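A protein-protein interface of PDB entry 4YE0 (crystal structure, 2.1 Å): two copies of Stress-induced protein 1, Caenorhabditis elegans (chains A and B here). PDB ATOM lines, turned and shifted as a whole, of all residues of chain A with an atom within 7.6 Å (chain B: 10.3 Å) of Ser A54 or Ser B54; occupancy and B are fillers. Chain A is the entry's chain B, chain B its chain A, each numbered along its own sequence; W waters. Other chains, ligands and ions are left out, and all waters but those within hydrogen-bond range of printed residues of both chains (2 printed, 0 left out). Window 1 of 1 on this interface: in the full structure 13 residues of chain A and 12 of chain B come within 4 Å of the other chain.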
ATOM      1  N   GLY A   1      18.677   1.355 -10.470  1.00  0.00           N
ATOM      2  CA  GLY A   1      18.216   1.206  -9.061  1.00  0.00           C
ATOM      3  C   GLY A   1      17.402  -0.049  -8.816  1.00  0.00           C
ATOM      4  O   GLY A   1      16.305   0.027  -8.264  1.00  0.00           O
ATOM      5  N   PHE A  22      25.087   4.406 -12.324  1.00  0.00           N
ATOM      6  CA  PHE A  22      25.124   5.842 -12.049  1.00  0.00           C
ATOM      7  C   PHE A  22      26.268   6.191 -11.110  1.00  0.00           C
ATOM      8  O   PHE A  22      26.561   5.448 -10.176  1.00  0.00           O
ATOM      9  CB  PHE A  22      23.803   6.292 -11.422  1.00  0.00           C
ATOM     10  CG  PHE A  22      22.605   6.013 -12.278  1.00  0.00           C
ATOM     11  CD1 PHE A  22      21.969   4.777 -12.222  1.00  0.00           C
ATOM     12  CD2 PHE A  22      22.119   6.977 -13.150  1.00  0.00           C
ATOM     13  CE1 PHE A  22      20.870   4.513 -13.019  1.00  0.00           C
ATOM     14  CE2 PHE A  22      21.018   6.719 -13.947  1.00  0.00           C
ATOM     15  CZ  PHE A  22      20.392   5.485 -13.880  1.00  0.00           C
ATOM     16  N   GLU A  39      16.763   8.566  -6.748  1.00  0.00           N
ATOM     17  CA  GLU A  39      16.740   8.860  -8.174  1.00  0.00           C
ATOM     18  C   GLU A  39      18.132   8.888  -8.750  1.00  0.00           C
ATOM     19  O   GLU A  39      19.071   9.360  -8.108  1.00  0.00           O
ATOM     20  CB  GLU A  39      16.090  10.216  -8.455  1.00  0.00           C
ATOM     21  CG  GLU A  39      14.904  10.562  -7.572  1.00  0.00           C
ATOM     22  CD  GLU A  39      14.230  11.857  -7.994  1.00  0.00           C
ATOM     23  OE1 GLU A  39      14.517  12.359  -9.105  1.00  0.00           O
ATOM     24  OE2 GLU A  39      13.407  12.374  -7.209  1.00  0.00           O
ATOM     25  N   GLY A  40      18.242   8.401  -9.981  1.00  0.00           N
ATOM     26  CA  GLY A  40      19.471   8.480 -10.754  1.00  0.00           C
ATOM     27  C   GLY A  40      19.166   9.134 -12.086  1.00  0.00           C
ATOM     28  O   GLY A  40      18.121   8.879 -12.678  1.00  0.00           O
ATOM     29  N   HIS A  41      20.057  10.003 -12.543  1.00  0.00           N
ATOM     30  CA  HIS A  41      19.957  10.564 -13.881  1.00  0.00           C
ATOM     31  C   HIS A  41      21.341  10.679 -14.494  1.00  0.00           C
ATOM     32  O   HIS A  41      22.219  11.341 -13.941  1.00  0.00           O
ATOM     33  CB  HIS A  41      19.266  11.930 -13.870  1.00  0.00           C
ATOM     34  CG  HIS A  41      18.961  12.456 -15.240  1.00  0.00           C
ATOM     35  ND1 HIS A  41      17.972  11.923 -16.038  1.00  0.00           N
ATOM     36  CD2 HIS A  41      19.524  13.457 -15.958  1.00  0.00           C
ATOM     37  CE1 HIS A  41      17.935  12.576 -17.186  1.00  0.00           C
ATOM     38  NE2 HIS A  41      18.865  13.511 -17.163  1.00  0.00           N
ATOM     39  N   HIS A  42      21.530  10.012 -15.628  1.00  0.00           N
ATOM     40  CA  HIS A  42      22.760  10.093 -16.397  1.00  0.00           C
ATOM     41  C   HIS A  42      22.393  10.575 -17.793  1.00  0.00           C
ATOM     42  O   HIS A  42      21.367  10.168 -18.342  1.00  0.00           O
ATOM     43  CB  HIS A  42      23.452   8.729 -16.450  1.00  0.00           C
ATOM     44  CG  HIS A  42      24.525   8.631 -17.491  1.00  0.00           C
ATOM     45  ND1 HIS A  42      25.862   8.804 -17.204  1.00  0.00           N
ATOM     46  CD2 HIS A  42      24.454   8.380 -18.820  1.00  0.00           C
ATOM     47  CE1 HIS A  42      26.570   8.663 -18.312  1.00  0.00           C
ATOM     48  NE2 HIS A  42      25.739   8.405 -19.306  1.00  0.00           N
ATOM     49  N   GLU A  43      23.223  11.444 -18.359  1.00  0.00           N
ATOM     50  CA  GLU A  43      22.905  12.080 -19.632  1.00  0.00           C
ATOM     51  C   GLU A  43      24.169  12.562 -20.334  1.00  0.00           C
ATOM     52  O   GLU A  43      24.774  13.559 -19.937  1.00  0.00           O
ATOM     53  CB  GLU A  43      21.931  13.238 -19.402  1.00  0.00           C
ATOM     54  CG  GLU A  43      21.347  13.838 -20.670  1.00  0.00           C
ATOM     55  CD  GLU A  43      20.101  14.670 -20.408  1.00  0.00           C
ATOM     56  OE1 GLU A  43      19.788  14.941 -19.228  1.00  0.00           O
ATOM     57  OE2 GLU A  43      19.430  15.056 -21.387  1.00  0.00           O
ATOM     58  N   LYS A  52      21.118   8.455 -22.411  1.00  0.00           N
ATOM     59  CA  LYS A  52      20.364   8.946 -21.276  1.00  0.00           C
ATOM     60  C   LYS A  52      19.824   7.759 -20.477  1.00  0.00           C
ATOM     61  O   LYS A  52      19.223   6.850 -21.046  1.00  0.00           O
ATOM     62  CB  LYS A  52      19.231   9.826 -21.798  1.00  0.00           C
ATOM     63  CG  LYS A  52      18.370  10.502 -20.749  1.00  0.00           C
ATOM     64  CD  LYS A  52      17.284  11.325 -21.432  1.00  0.00           C
ATOM     65  CE  LYS A  52      16.146  11.655 -20.481  1.00  0.00           C
ATOM     66  NZ  LYS A  52      15.292  12.760 -20.996  1.00  0.00           N
ATOM     67  N   ARG A  53      20.071   7.766 -19.168  1.00  0.00           N
ATOM     68  CA  ARG A  53      19.529   6.761 -18.250  1.00  0.00           C
ATOM     69  C   ARG A  53      18.891   7.444 -17.057  1.00  0.00           C
ATOM     70  O   ARG A  53      19.316   8.531 -16.652  1.00  0.00           O
ATOM     71  CB  ARG A  53      20.627   5.832 -17.742  1.00  0.00           C
ATOM     72  CG  ARG A  53      20.997   4.724 -18.700  1.00  0.00           C
ATOM     73  CD  ARG A  53      21.871   3.683 -18.014  1.00  0.00           C
ATOM     74  NE  ARG A  53      23.076   4.255 -17.414  1.00  0.00           N
ATOM     75  CZ  ARG A  53      24.125   4.706 -18.100  1.00  0.00           C
ATOM     76  NH1 ARG A  53      25.174   5.196 -17.452  1.00  0.00           N
ATOM     77  NH2 ARG A  53      24.140   4.685 -19.430  1.00  0.00           N
ATOM     78  N   SER A  54      17.881   6.796 -16.484  1.00  0.00           N
ATOM     79  CA  SER A  54      17.153   7.361 -15.362  1.00  0.00           C
ATOM     80  C   SER A  54      16.418   6.293 -14.581  1.00  0.00           C
ATOM     81  O   SER A  54      16.014   5.267 -15.131  1.00  0.00           O
ATOM     82  CB  SER A  54      16.138   8.398 -15.846  1.00  0.00           C
ATOM     83  OG  SER A  54      16.781   9.497 -16.468  1.00  0.00           O
ATOM     84  N   PHE A  55      16.253   6.543 -13.288  1.00  0.00           N
ATOM     85  CA  PHE A  55      15.328   5.762 -12.489  1.00  0.00           C
ATOM     86  C   PHE A  55      14.839   6.590 -11.313  1.00  0.00           C
ATOM     87  O   PHE A  55      15.520   7.507 -10.859  1.00  0.00           O
ATOM     88  CB  PHE A  55      15.962   4.443 -12.019  1.00  0.00           C
ATOM     89  CG  PHE A  55      16.778   4.567 -10.765  1.00  0.00           C
ATOM     90  CD1 PHE A  55      18.124   4.892 -10.831  1.00  0.00           C
ATOM     91  CD2 PHE A  55      16.201   4.356  -9.518  1.00  0.00           C
ATOM     92  CE1 PHE A  55      18.879   5.004  -9.681  1.00  0.00           C
ATOM     93  CE2 PHE A  55      16.952   4.476  -8.362  1.00  0.00           C
ATOM     94  CZ  PHE A  55      18.294   4.797  -8.444  1.00  0.00           C
ATOM     95  N   THR A  56      13.635   6.274 -10.858  1.00  0.00           N
ATOM     96  CA  THR A  56      13.089   6.814  -9.629  1.00  0.00           C
ATOM     97  C   THR A  56      12.496   5.643  -8.867  1.00  0.00           C
ATOM     98  O   THR A  56      11.682   4.895  -9.413  1.00  0.00           O
ATOM     99  CB  THR A  56      11.987   7.857  -9.903  1.00  0.00           C
ATOM    100  OG1 THR A  56      12.515   8.913 -10.711  1.00  0.00           O
ATOM    101  CG2 THR A  56      11.458   8.445  -8.600  1.00  0.00           C
ATOM    102  N   GLY B   1      20.632   0.565 -21.043  1.00  0.00           N
ATOM    103  CA  GLY B   1      20.760   0.428 -22.533  1.00  0.00           C
ATOM    104  C   GLY B   1      22.210   0.491 -22.982  1.00  0.00           C
ATOM    105  O   GLY B   1      22.571   1.306 -23.833  1.00  0.00           O
ATOM    106  N   SER B   2      23.021  -0.412 -22.436  1.00  0.00           N
ATOM    107  CA  SER B   2      24.480  -0.242 -22.337  1.00  0.00           C
ATOM    108  C   SER B   2      25.301  -0.129 -23.633  1.00  0.00           C
ATOM    109  O   SER B   2      26.411   0.402 -23.595  1.00  0.00           O
ATOM    110  CB  SER B   2      25.059  -1.369 -21.474  1.00  0.00           C
ATOM    111  OG  SER B   2      24.420  -1.412 -20.209  1.00  0.00           O
ATOM    112  N   ASP B  18      22.289  -3.800 -24.282  1.00  0.00           N
ATOM    113  CA  ASP B  18      21.819  -4.531 -23.111  1.00  0.00           C
ATOM    114  C   ASP B  18      20.449  -3.969 -22.741  1.00  0.00           C
ATOM    115  O   ASP B  18      20.329  -2.827 -22.302  1.00  0.00           O
ATOM    116  CB  ASP B  18      22.798  -4.379 -21.942  1.00  0.00           C
ATOM    117  CG  ASP B  18      22.455  -5.279 -20.760  1.00  0.00           C
ATOM    118  OD1 ASP B  18      23.314  -5.427 -19.866  1.00  0.00           O
ATOM    119  OD2 ASP B  18      21.337  -5.840 -20.718  1.00  0.00           O
ATOM    120  N   VAL B  19      19.427  -4.799 -22.909  1.00  0.00           N
ATOM    121  CA  VAL B  19      18.040  -4.364 -22.862  1.00  0.00           C
ATOM    122  C   VAL B  19      17.220  -5.231 -21.879  1.00  0.00           C
ATOM    123  O   VAL B  19      15.989  -5.153 -21.829  1.00  0.00           O
ATOM    124  CB  VAL B  19      17.517  -4.339 -24.330  1.00  0.00           C
ATOM    125  CG1 VAL B  19      16.137  -4.939 -24.509  1.00  0.00           C
ATOM    126  CG2 VAL B  19      17.594  -2.924 -24.891  1.00  0.00           C
ATOM    127  N   ALA B  21      16.725  -5.205 -18.642  1.00  0.00           N
ATOM    128  CA  ALA B  21      15.977  -4.578 -17.550  1.00  0.00           C
ATOM    129  C   ALA B  21      14.550  -4.200 -17.945  1.00  0.00           C
ATOM    130  O   ALA B  21      13.778  -3.741 -17.101  1.00  0.00           O
ATOM    131  CB  ALA B  21      16.717  -3.346 -17.045  1.00  0.00           C
ATOM    132  N   PHE B  22      14.204  -4.382 -19.218  1.00  0.00           N
ATOM    133  CA  PHE B  22      12.900  -3.983 -19.735  1.00  0.00           C
ATOM    134  C   PHE B  22      12.212  -5.138 -20.426  1.00  0.00           C
ATOM    135  O   PHE B  22      12.862  -6.013 -20.993  1.00  0.00           O
ATOM    136  CB  PHE B  22      13.063  -2.830 -20.728  1.00  0.00           C
ATOM    137  CG  PHE B  22      13.675  -1.611 -20.120  1.00  0.00           C
ATOM    138  CD1 PHE B  22      15.050  -1.510 -19.980  1.00  0.00           C
ATOM    139  CD2 PHE B  22      12.874  -0.581 -19.648  1.00  0.00           C
ATOM    140  CE1 PHE B  22      15.618  -0.398 -19.389  1.00  0.00           C
ATOM    141  CE2 PHE B  22      13.438   0.537 -19.063  1.00  0.00           C
ATOM    142  CZ  PHE B  22      14.808   0.630 -18.933  1.00  0.00           C
ATOM    143  N   GLU B  26       7.981  -2.668 -23.424  1.00  0.00           N
ATOM    144  CA  GLU B  26       8.434  -1.392 -22.877  1.00  0.00           C
ATOM    145  C   GLU B  26       9.533  -0.756 -23.730  1.00  0.00           C
ATOM    146  O   GLU B  26      10.153   0.221 -23.308  1.00  0.00           O
ATOM    147  CB  GLU B  26       8.947  -1.604 -21.454  1.00  0.00           C
ATOM    148  CG  GLU B  26       7.866  -1.992 -20.456  1.00  0.00           C
ATOM    149  CD  GLU B  26       8.428  -2.477 -19.128  1.00  0.00           C
ATOM    150  OE1 GLU B  26       9.625  -2.832 -19.062  1.00  0.00           O
ATOM    151  OE2 GLU B  26       7.666  -2.507 -18.141  1.00  0.00           O
ATOM    152  N   LEU B  27       9.767  -1.295 -24.925  1.00  0.00           N
ATOM    153  CA  LEU B  27      10.842  -0.825 -25.783  1.00  0.00           C
ATOM    154  C   LEU B  27      10.328  -0.249 -27.089  1.00  0.00           C
ATOM    155  O   LEU B  27       9.361  -0.746 -27.663  1.00  0.00           O
ATOM    156  CB  LEU B  27      11.821  -1.960 -26.062  1.00  0.00           C
ATOM    157  CG  LEU B  27      12.618  -2.370 -24.826  1.00  0.00           C
ATOM    158  CD1 LEU B  27      13.159  -3.778 -24.997  1.00  0.00           C
ATOM    159  CD2 LEU B  27      13.745  -1.379 -24.539  1.00  0.00           C
ATOM    160  N   ILE B  38      16.611   4.346 -29.665  1.00  0.00           N
ATOM    161  CA  ILE B  38      16.103   3.224 -28.882  1.00  0.00           C
ATOM    162  C   ILE B  38      15.721   3.716 -27.496  1.00  0.00           C
ATOM    163  O   ILE B  38      16.540   4.320 -26.801  1.00  0.00           O
ATOM    164  CB  ILE B  38      17.145   2.100 -28.727  1.00  0.00           C
ATOM    165  CG1 ILE B  38      17.645   1.637 -30.100  1.00  0.00           C
ATOM    166  CG2 ILE B  38      16.555   0.940 -27.937  1.00  0.00           C
ATOM    167  CD1 ILE B  38      18.889   2.354 -30.577  1.00  0.00           C
ATOM    168  N   GLU B  39      14.484   3.432 -27.095  1.00  0.00           N
ATOM    169  CA  GLU B  39      13.935   3.897 -25.826  1.00  0.00           C
ATOM    170  C   GLU B  39      13.336   2.753 -25.024  1.00  0.00           C
ATOM    171  O   GLU B  39      12.712   1.851 -25.579  1.00  0.00           O
ATOM    172  CB  GLU B  39      12.839   4.939 -26.069  1.00  0.00           C
ATOM    173  CG  GLU B  39      13.365   6.326 -26.376  1.00  0.00           C
ATOM    174  CD  GLU B  39      12.257   7.350 -26.540  1.00  0.00           C
ATOM    175  OE1 GLU B  39      11.287   7.329 -25.751  1.00  0.00           O
ATOM    176  OE2 GLU B  39      12.361   8.187 -27.460  1.00  0.00           O
ATOM    177  N   GLY B  40      13.518   2.819 -23.712  1.00  0.00           N
ATOM    178  CA  GLY B  40      12.892   1.889 -22.785  1.00  0.00           C
ATOM    179  C   GLY B  40      12.238   2.665 -21.660  1.00  0.00           C
ATOM    180  O   GLY B  40      12.839   3.593 -21.118  1.00  0.00           O
ATOM    181  N   HIS B  41      11.002   2.310 -21.324  1.00  0.00           N
ATOM    182  CA  HIS B  41      10.323   2.907 -20.182  1.00  0.00           C
ATOM    183  C   HIS B  41       9.583   1.850 -19.379  1.00  0.00           C
ATOM    184  O   HIS B  41       8.676   1.185 -19.887  1.00  0.00           O
ATOM    185  CB  HIS B  41       9.360   4.014 -20.610  1.00  0.00           C
ATOM    186  CG  HIS B  41       8.767   4.767 -19.457  1.00  0.00           C
ATOM    187  ND1 HIS B  41       7.455   5.190 -19.432  1.00  0.00           N
ATOM    188  CD2 HIS B  41       9.305   5.148 -18.275  1.00  0.00           C
ATOM    189  CE1 HIS B  41       7.217   5.813 -18.292  1.00  0.00           C
ATOM    190  NE2 HIS B  41       8.324   5.801 -17.571  1.00  0.00           N
ATOM    191  N   HIS B  42       9.991   1.694 -18.125  1.00  0.00           N
ATOM    192  CA  HIS B  42       9.309   0.818 -17.191  1.00  0.00           C
ATOM    193  C   HIS B  42       8.797   1.660 -16.027  1.00  0.00           C
ATOM    194  O   HIS B  42       9.543   2.454 -15.454  1.00  0.00           O
ATOM    195  CB  HIS B  42      10.259  -0.268 -16.695  1.00  0.00           C
ATOM    196  CG  HIS B  42       9.759  -0.994 -15.489  1.00  0.00           C
ATOM    197  ND1 HIS B  42       8.871  -2.046 -15.569  1.00  0.00           N
ATOM    198  CD2 HIS B  42      10.009  -0.811 -14.172  1.00  0.00           C
ATOM    199  CE1 HIS B  42       8.600  -2.483 -14.352  1.00  0.00           C
ATOM    200  NE2 HIS B  42       9.278  -1.750 -13.487  1.00  0.00           N
ATOM    201  N   GLU B  43       7.524   1.478 -15.689  1.00  0.00           N
ATOM    202  CA  GLU B  43       6.871   2.250 -14.640  1.00  0.00           C
ATOM    203  C   GLU B  43       5.879   1.354 -13.908  1.00  0.00           C
ATOM    204  O   GLU B  43       4.861   0.949 -14.474  1.00  0.00           O
ATOM    205  CB  GLU B  43       6.158   3.456 -15.250  1.00  0.00           C
ATOM    206  CG  GLU B  43       5.534   4.406 -14.240  1.00  0.00           C
ATOM    207  CD  GLU B  43       5.069   5.704 -14.874  1.00  0.00           C
ATOM    208  OE1 GLU B  43       4.646   5.681 -16.051  1.00  0.00           O
ATOM    209  OE2 GLU B  43       5.121   6.751 -14.193  1.00  0.00           O
ATOM    210  N   VAL B  44       6.191   1.041 -12.652  1.00  0.00           N
ATOM    211  CA  VAL B  44       5.394   0.122 -11.843  1.00  0.00           C
ATOM    212  C   VAL B  44       4.890   0.820 -10.584  1.00  0.00           C
ATOM    213  O   VAL B  44       5.564   1.691 -10.041  1.00  0.00           O
ATOM    214  CB  VAL B  44       6.215  -1.150 -11.490  1.00  0.00           C
ATOM    215  CG1 VAL B  44       6.257  -1.428  -9.986  1.00  0.00           C
ATOM    216  CG2 VAL B  44       5.678  -2.355 -12.251  1.00  0.00           C
ATOM    217  N   PHE B  50       6.705   3.209  -5.455  1.00  0.00           N
ATOM    218  CA  PHE B  50       6.753   2.848  -6.873  1.00  0.00           C
ATOM    219  C   PHE B  50       8.171   2.763  -7.433  1.00  0.00           C
ATOM    220  O   PHE B  50       9.132   3.200  -6.803  1.00  0.00           O
ATOM    221  CB  PHE B  50       5.900   3.815  -7.711  1.00  0.00           C
ATOM    222  CG  PHE B  50       6.564   5.130  -8.002  1.00  0.00           C
ATOM    223  CD1 PHE B  50       7.404   5.270  -9.101  1.00  0.00           C
ATOM    224  CD2 PHE B  50       6.332   6.234  -7.195  1.00  0.00           C
ATOM    225  CE1 PHE B  50       8.014   6.481  -9.378  1.00  0.00           C
ATOM    226  CE2 PHE B  50       6.938   7.450  -7.467  1.00  0.00           C
ATOM    227  CZ  PHE B  50       7.781   7.573  -8.560  1.00  0.00           C
ATOM    228  N   SER B  51       8.272   2.188  -8.628  1.00  0.00           N
ATOM    229  CA  SER B  51       9.536   2.027  -9.332  1.00  0.00           C
ATOM    230  C   SER B  51       9.394   2.482 -10.778  1.00  0.00           C
ATOM    231  O   SER B  51       8.371   2.248 -11.425  1.00  0.00           O
ATOM    232  CB  SER B  51       9.989   0.571  -9.296  1.00  0.00           C
ATOM    233  OG  SER B  51      11.146   0.390 -10.091  1.00  0.00           O
ATOM    234  N   LYS B  52      10.443   3.114 -11.284  1.00  0.00           N
ATOM    235  CA  LYS B  52      10.409   3.750 -12.587  1.00  0.00           C
ATOM    236  C   LYS B  52      11.821   3.710 -13.171  1.00  0.00           C
ATOM    237  O   LYS B  52      12.781   4.063 -12.492  1.00  0.00           O
ATOM    238  CB  LYS B  52       9.895   5.181 -12.411  1.00  0.00           C
ATOM    239  CG  LYS B  52       9.840   6.048 -13.659  1.00  0.00           C
ATOM    240  CD  LYS B  52       9.423   7.467 -13.271  1.00  0.00           C
ATOM    241  CE  LYS B  52       9.731   8.496 -14.352  1.00  0.00           C
ATOM    242  NZ  LYS B  52       8.548   8.794 -15.213  1.00  0.00           N
ATOM    243  N   ARG B  53      11.934   3.244 -14.413  1.00  0.00           N
ATOM    244  CA  ARG B  53      13.210   3.115 -15.115  1.00  0.00           C
ATOM    245  C   ARG B  53      13.043   3.619 -16.529  1.00  0.00           C
ATOM    246  O   ARG B  53      11.964   3.523 -17.104  1.00  0.00           O
ATOM    247  CB  ARG B  53      13.646   1.656 -15.210  1.00  0.00           C
ATOM    248  CG  ARG B  53      14.259   1.073 -13.960  1.00  0.00           C
ATOM    249  CD  ARG B  53      14.943  -0.248 -14.284  1.00  0.00           C
ATOM    250  NE  ARG B  53      14.021  -1.280 -14.754  1.00  0.00           N
ATOM    251  CZ  ARG B  53      13.191  -1.966 -13.971  1.00  0.00           C
ATOM    252  NH1 ARG B  53      13.129  -1.727 -12.667  1.00  0.00           N
ATOM    253  NH2 ARG B  53      12.400  -2.897 -14.492  1.00  0.00           N
ATOM    254  N   SER B  54      14.133   4.111 -17.100  1.00  0.00           N
ATOM    255  CA  SER B  54      14.101   4.725 -18.413  1.00  0.00           C
ATOM    256  C   SER B  54      15.483   4.742 -19.021  1.00  0.00           C
ATOM    257  O   SER B  54      16.486   4.820 -18.306  1.00  0.00           O
ATOM    258  CB  SER B  54      13.601   6.167 -18.312  1.00  0.00           C
ATOM    259  OG  SER B  54      12.198   6.217 -18.169  1.00  0.00           O
ATOM    260  N   PHE B  55      15.530   4.670 -20.344  1.00  0.00           N
ATOM    261  CA  PHE B  55      16.739   5.009 -21.073  1.00  0.00           C
ATOM    262  C   PHE B  55      16.388   5.434 -22.490  1.00  0.00           C
ATOM    263  O   PHE B  55      15.347   5.053 -23.031  1.00  0.00           O
ATOM    264  CB  PHE B  55      17.759   3.856 -21.065  1.00  0.00           C
ATOM    265  CG  PHE B  55      17.579   2.864 -22.181  1.00  0.00           C
ATOM    266  CD1 PHE B  55      16.797   1.729 -21.999  1.00  0.00           C
ATOM    267  CD2 PHE B  55      18.206   3.053 -23.408  1.00  0.00           C
ATOM    268  CE1 PHE B  55      16.634   0.811 -23.024  1.00  0.00           C
ATOM    269  CE2 PHE B  55      18.045   2.138 -24.435  1.00  0.00           C
ATOM    270  CZ  PHE B  55      17.259   1.014 -24.242  1.00  0.00           C
ATOM    271  N   THR B  56      17.257   6.254 -23.064  1.00  0.00           N
ATOM    272  CA  THR B  56      17.150   6.657 -24.449  1.00  0.00           C
ATOM    273  C   THR B  56      18.551   6.626 -25.035  1.00  0.00           C
ATOM    274  O   THR B  56      19.464   7.266 -24.514  1.00  0.00           O
ATOM    275  CB  THR B  56      16.546   8.066 -24.581  1.00  0.00           C
ATOM    276  OG1 THR B  56      15.325   8.131 -23.840  1.00  0.00           O
ATOM    277  CG2 THR B  56      16.267   8.408 -26.046  1.00  0.00           C
ATOM    278  N   ARG B  57      18.723   5.852 -26.100  1.00  0.00           N
ATOM    279  CA  ARG B  57      19.995   5.761 -26.802  1.00  0.00           C
ATOM    280  C   ARG B  57      19.750   6.200 -28.229  1.00  0.00           C
ATOM    281  O   ARG B  57      18.810   5.741 -28.877  1.00  0.00           O
ATOM    282  CB  ARG B  57      20.518   4.327 -26.775  1.00  0.00           C
ATOM    283  CG  ARG B  57      21.823   4.104 -27.529  1.00  0.00           C
ATOM    284  CD  ARG B  57      23.049   4.512 -26.728  1.00  0.00           C
ATOM    285  NE  ARG B  57      23.160   3.790 -25.462  1.00  0.00           N
ATOM    286  CZ  ARG B  57      24.160   3.936 -24.595  1.00  0.00           C
ATOM    287  NH1 ARG B  57      24.163   3.237 -23.467  1.00  0.00           N
ATOM    288  NH2 ARG B  57      25.162   4.770 -24.844  1.00  0.00           N
HETATM  289  O   HOH W   1      21.039   5.121 -22.738  1.00  0.00           O
HETATM  290  O   HOH W   2      12.917   6.843 -15.081  1.00  0.00           O
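Lys A52 touches Phe B55, and with the chains exchanged Phe A55 touches Lys B52. Lys A52 touches Thr B56, and with the chains exchanged Thr A56 touches Lys B52. Arg A53 touches Ser B54, and with the chains exchanged Ser A54 touches Arg B53. Ser B54 touches its own counterpart, Ser A54. Of the 9 pairs that touch across the chains among the printed residues, 7 have their exchanged pair printed and touching as well.
No residue of chain B comes within 4 Å of Gly A40. Of the printed residues of chain B, Arg A53 touches Ser B54 (3.6 Å). Of the printed residues of chain B, Phe A55 touches Lys B52 (3.1 Å). Printed residues of chain A within 4 Å of Phe B50: Thr A56 (3.8 Å). Printed residues of chain A within 4 Å of Lys B52: Phe A55 (3.1 Å) and Thr A56 (2.9 Å). Of the printed residues of chain A, Arg B53 touches Ser A54 (3.5 Å). Of chain A, only Arg A53 (3.6 Å) and Ser A54 (3.0 Å) come within 4 Å of Ser B54. The nearest printed residue of chain A that does not touch Phe B50 is Phe A55 (7.1 Å).
The backbone NH (N) of Lys B52 sits at hydrogen-bond distance from the backbone carbonyl oxygen (O) of Thr A56. The backbone NH (N) of Ser B54 sits at hydrogen-bond distance from the backbone carbonyl oxygen (O) of Ser A54 (3.0 Å). N of Thr B56 lies within hydrogen-bond range of O of Lys A52 (2.9 Å).
Of the 23 printed residues of chain B, 7 touch a printed residue of chain A. Printed residues of chain B that touch a printed residue of chain A: Phe B50, Ser B51, Lys B52, Arg B53, Ser B54, Phe B55 and Thr B56. Hydrophobic or aromatic side chains of chain B within 4 Å of the printed part of chain A: Phe B50 and Phe B55. Of the 12 printed residues of chain A, 5 touch a printed residue of chain B. Hydrophobic or aromatic side chains of chain A that line the printed part of chain B: Phe A55. Among the printed residues, 9 pairs touch across the chains. Among the printed residues, no Asp or Glu carboxylate lies within 4 Å of a Lys or Arg side-chain nitrogen of the other chain.
Phe B55 touches Lys A52 (CA to O, 3.1 Å). Arg A53 touches Ser B54. Arg B53 touches Ser A54 (CA to O, 3.5 Å). Phe A55 touches Lys B52. CG2 of Thr A56 touches CZ of Phe B50, 3.8 Å away. Ser B51 touches Thr A56.
The backbone NH (N) of Gly B40 lies within hydrogen-bond range of the backbone carbonyl oxygen (O) of Phe B55. The backbone NH (N) of Arg B53 sits at hydrogen-bond distance from the backbone carbonyl oxygen (O) of His B42 (2.7 Å). The backbone NH of Val B44 is in hydrogen-bond range of the backbone carbonyl oxygen of Ser B51 (2.8 Å). The backbone carbonyl oxygen (O) of Phe A55 sits at hydrogen-bond distance from the backbone NH (N) of Gly A40 (3.0 Å). The side-chain hydroxyl (OG) of Ser A54 sits at hydrogen-bond distance from a ring nitrogen (ND1) of His A41 (2.7 Å). The backbone carbonyl oxygen of His A42 lies within hydrogen-bond range of the backbone NH of Arg A53, 2.9 Å away.
Water W1 bridges the backbone carbonyl oxygen of Lys A52 (3.0 Å) and the backbone carbonyl oxygen of Thr B56 (3.2 Å). Water W2 bridges OG of Ser B54 and O of Ser A54.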
